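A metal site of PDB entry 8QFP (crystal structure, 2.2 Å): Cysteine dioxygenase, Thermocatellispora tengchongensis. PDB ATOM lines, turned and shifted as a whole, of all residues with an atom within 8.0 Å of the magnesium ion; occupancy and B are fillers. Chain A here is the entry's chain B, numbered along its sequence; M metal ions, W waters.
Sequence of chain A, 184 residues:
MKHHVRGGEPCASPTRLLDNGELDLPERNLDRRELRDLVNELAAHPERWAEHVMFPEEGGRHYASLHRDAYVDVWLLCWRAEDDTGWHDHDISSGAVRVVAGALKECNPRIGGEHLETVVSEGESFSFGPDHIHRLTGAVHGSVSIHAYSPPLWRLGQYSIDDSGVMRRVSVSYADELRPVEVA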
ATOM      1  N   GLY A  21       4.984  -3.998  11.487  1.00  0.00           N
ATOM      2  CA  GLY A  21       5.303  -3.956  10.076  1.00  0.00           C
ATOM      3  C   GLY A  21       6.023  -5.214   9.665  1.00  0.00           C
ATOM      4  O   GLY A  21       6.761  -5.789  10.456  1.00  0.00           O
ATOM      5  N   GLU A  22       5.810  -5.644   8.416  1.00  0.00           N
ATOM      6  CA  GLU A  22       6.351  -6.903   7.939  1.00  0.00           C
ATOM      7  C   GLU A  22       7.843  -6.983   8.204  1.00  0.00           C
ATOM      8  O   GLU A  22       8.549  -5.977   8.147  1.00  0.00           O
ATOM      9  CB  GLU A  22       6.068  -7.077   6.444  1.00  0.00           C
ATOM     10  CG  GLU A  22       6.210  -8.525   5.958  1.00  0.00           C
ATOM     11  CD  GLU A  22       5.597  -9.536   6.917  1.00  0.00           C
ATOM     12  OE1 GLU A  22       4.352  -9.658   6.962  1.00  0.00           O
ATOM     13  OE2 GLU A  22       6.359 -10.206   7.638  1.00  0.00           O
ATOM     14  N   LEU A  23       8.326  -8.199   8.507  1.00  0.00           N
ATOM     15  CA  LEU A  23       9.734  -8.454   8.772  1.00  0.00           C
ATOM     16  C   LEU A  23      10.241  -9.509   7.810  1.00  0.00           C
ATOM     17  O   LEU A  23       9.610 -10.564   7.643  1.00  0.00           O
ATOM     18  CB  LEU A  23       9.956  -8.921  10.222  1.00  0.00           C
ATOM     19  CG  LEU A  23       9.741  -7.914  11.357  1.00  0.00           C
ATOM     20  CD1 LEU A  23       9.884  -8.598  12.709  1.00  0.00           C
ATOM     21  CD2 LEU A  23      10.707  -6.733  11.238  1.00  0.00           C
ATOM     22  N   ASP A  24      11.375  -9.233   7.188  1.00  0.00           N
ATOM     23  CA  ASP A  24      12.024 -10.157   6.255  1.00  0.00           C
ATOM     24  C   ASP A  24      12.663 -11.296   7.053  1.00  0.00           C
ATOM     25  O   ASP A  24      13.811 -11.188   7.511  1.00  0.00           O
ATOM     26  CB  ASP A  24      13.064  -9.410   5.423  1.00  0.00           C
ATOM     27  CG  ASP A  24      13.560 -10.223   4.236  1.00  0.00           C
ATOM     28  OD1 ASP A  24      13.342 -11.455   4.202  1.00  0.00           O
ATOM     29  OD2 ASP A  24      14.180  -9.624   3.331  1.00  0.00           O
ATOM     30  N   LEU A  25      11.929 -12.400   7.205  1.00  0.00           N
ATOM     31  CA  LEU A  25      12.348 -13.547   7.987  1.00  0.00           C
ATOM     32  C   LEU A  25      12.097 -14.826   7.209  1.00  0.00           C
ATOM     33  O   LEU A  25      11.233 -14.869   6.332  1.00  0.00           O
ATOM     34  CB  LEU A  25      11.566 -13.622   9.312  1.00  0.00           C
ATOM     35  CG  LEU A  25      11.866 -12.500  10.320  1.00  0.00           C
ATOM     36  CD1 LEU A  25      10.848 -12.492  11.441  1.00  0.00           C
ATOM     37  CD2 LEU A  25      13.290 -12.642  10.857  1.00  0.00           C
ATOM     38  N   PRO A  26      12.855 -15.887   7.491  1.00  0.00           N
ATOM     39  CA  PRO A  26      12.499 -17.193   6.923  1.00  0.00           C
ATOM     40  C   PRO A  26      11.060 -17.529   7.265  1.00  0.00           C
ATOM     41  O   PRO A  26      10.525 -17.113   8.306  1.00  0.00           O
ATOM     42  CB  PRO A  26      13.488 -18.153   7.609  1.00  0.00           C
ATOM     43  CG  PRO A  26      14.621 -17.274   8.059  1.00  0.00           C
ATOM     44  CD  PRO A  26      14.001 -15.965   8.402  1.00  0.00           C
ATOM     45  N   GLU A  27      10.404 -18.270   6.363  1.00  0.00           N
ATOM     46  CA  GLU A  27       9.007 -18.663   6.537  1.00  0.00           C
ATOM     47  C   GLU A  27       8.922 -19.981   7.317  1.00  0.00           C
ATOM     48  O   GLU A  27       8.567 -21.035   6.794  1.00  0.00           O
ATOM     49  CB  GLU A  27       8.324 -18.774   5.178  1.00  0.00           C
ATOM     50  CG  GLU A  27       8.224 -17.460   4.404  1.00  0.00           C
ATOM     51  CD  GLU A  27       9.528 -17.033   3.763  1.00  0.00           C
ATOM     52  OE1 GLU A  27      10.479 -17.854   3.689  1.00  0.00           O
ATOM     53  OE2 GLU A  27       9.609 -15.871   3.313  1.00  0.00           O
ATOM     54  N   HIS A  67       5.372  -6.961  15.637  1.00  0.00           N
ATOM     55  CA  HIS A  67       4.943  -7.838  14.557  1.00  0.00           C
ATOM     56  C   HIS A  67       4.507  -9.190  15.106  1.00  0.00           C
ATOM     57  O   HIS A  67       5.200  -9.769  15.954  1.00  0.00           O
ATOM     58  CB  HIS A  67       6.068  -8.012  13.522  1.00  0.00           C
ATOM     59  CG  HIS A  67       5.637  -8.728  12.270  1.00  0.00           C
ATOM     60  ND1 HIS A  67       4.687  -8.219  11.407  1.00  0.00           N
ATOM     61  CD2 HIS A  67       6.036  -9.913  11.746  1.00  0.00           C
ATOM     62  CE1 HIS A  67       4.530  -9.056  10.399  1.00  0.00           C
ATOM     63  NE2 HIS A  67       5.324 -10.094  10.574  1.00  0.00           N
ATOM     64  N   ARG A  68       3.356  -9.670  14.660  1.00  0.00           N
ATOM     65  CA  ARG A  68       2.868 -11.010  14.966  1.00  0.00           C
ATOM     66  C   ARG A  68       2.409 -11.640  13.670  1.00  0.00           C
ATOM     67  O   ARG A  68       1.602 -11.052  12.940  1.00  0.00           O
ATOM     68  CB  ARG A  68       1.692 -10.973  15.951  1.00  0.00           C
ATOM     69  CG  ARG A  68       1.963 -10.204  17.225  1.00  0.00           C
ATOM     70  CD  ARG A  68       0.711 -10.177  18.107  1.00  0.00           C
ATOM     71  NE  ARG A  68       0.628 -11.364  18.967  1.00  0.00           N
ATOM     72  CZ  ARG A  68      -0.145 -12.410  18.721  1.00  0.00           C
ATOM     73  NH1 ARG A  68      -0.924 -12.420  17.644  1.00  0.00           N
ATOM     74  NH2 ARG A  68      -0.161 -13.450  19.564  1.00  0.00           N
ATOM     75  N   ASP A  69       2.937 -12.818  13.363  1.00  0.00           N
ATOM     76  CA  ASP A  69       2.440 -13.620  12.240  1.00  0.00           C
ATOM     77  C   ASP A  69       2.398 -15.068  12.720  1.00  0.00           C
ATOM     78  O   ASP A  69       2.304 -15.342  13.915  1.00  0.00           O
ATOM     79  CB  ASP A  69       3.289 -13.390  10.983  1.00  0.00           C
ATOM     80  CG  ASP A  69       4.754 -13.759  11.181  1.00  0.00           C
ATOM     81  OD1 ASP A  69       5.068 -14.523  12.110  1.00  0.00           O
ATOM     82  OD2 ASP A  69       5.596 -13.290  10.371  1.00  0.00           O
ATOM     83  N   ALA A  70       2.449 -16.006  11.764  1.00  0.00           N
ATOM     84  CA  ALA A  70       2.295 -17.421  12.066  1.00  0.00           C
ATOM     85  C   ALA A  70       3.540 -18.037  12.703  1.00  0.00           C
ATOM     86  O   ALA A  70       3.446 -19.135  13.252  1.00  0.00           O
ATOM     87  CB  ALA A  70       1.946 -18.202  10.790  1.00  0.00           C
ATOM     88  N   TYR A  71       4.682 -17.352  12.632  1.00  0.00           N
ATOM     89  CA  TYR A  71       5.960 -17.857  13.087  1.00  0.00           C
ATOM     90  C   TYR A  71       6.555 -17.089  14.240  1.00  0.00           C
ATOM     91  O   TYR A  71       7.190 -17.680  15.126  1.00  0.00           O
ATOM     92  CB  TYR A  71       6.974 -17.858  11.924  1.00  0.00           C
ATOM     93  CG  TYR A  71       6.410 -18.528  10.690  1.00  0.00           C
ATOM     94  CD1 TYR A  71       6.171 -19.920  10.659  1.00  0.00           C
ATOM     95  CD2 TYR A  71       6.099 -17.782   9.554  1.00  0.00           C
ATOM     96  CE1 TYR A  71       5.650 -20.540   9.531  1.00  0.00           C
ATOM     97  CE2 TYR A  71       5.580 -18.392   8.424  1.00  0.00           C
ATOM     98  CZ  TYR A  71       5.351 -19.755   8.405  1.00  0.00           C
ATOM     99  OH  TYR A  71       4.824 -20.333   7.261  1.00  0.00           O
ATOM    100  N   VAL A  72       6.369 -15.763  14.273  1.00  0.00           N
ATOM    101  CA  VAL A  72       7.078 -14.938  15.227  1.00  0.00           C
ATOM    102  C   VAL A  72       6.102 -14.022  15.952  1.00  0.00           C
ATOM    103  O   VAL A  72       4.984 -13.766  15.493  1.00  0.00           O
ATOM    104  CB  VAL A  72       8.189 -14.112  14.552  1.00  0.00           C
ATOM    105  CG1 VAL A  72       7.586 -12.887  13.895  1.00  0.00           C
ATOM    106  CG2 VAL A  72       9.243 -13.703  15.554  1.00  0.00           C
HETATM  107 MG    MG M   1       5.638 -11.688   9.053  1.00  0.00          MG
HETATM  108  O   HOH W   1       7.794 -11.981   9.300  1.00  0.00           O
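Within 4 Å of the magnesium ion: Glu 22, His 67 and Asp 69. The nearest printed residue that does not touch the magnesium ion is Leu 23 (4.4 Å).
The magnesium ion is bound by the side-chain carboxylate of Asp 69, the side-chain carboxylate of Glu 22, water W1 and a ring nitrogen (NE2) of His 67.
N of Tyr 71 is in hydrogen-bond range of OD1 of Asp 69 (2.9 Å). A ring nitrogen (ND1) of His 67 lies within hydrogen-bond range of the backbone carbonyl oxygen of Gly 21, at 3.3 Å. OD1 of Asp 69 lies within hydrogen-bond range of N of Val 72, 2.8 Å away.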
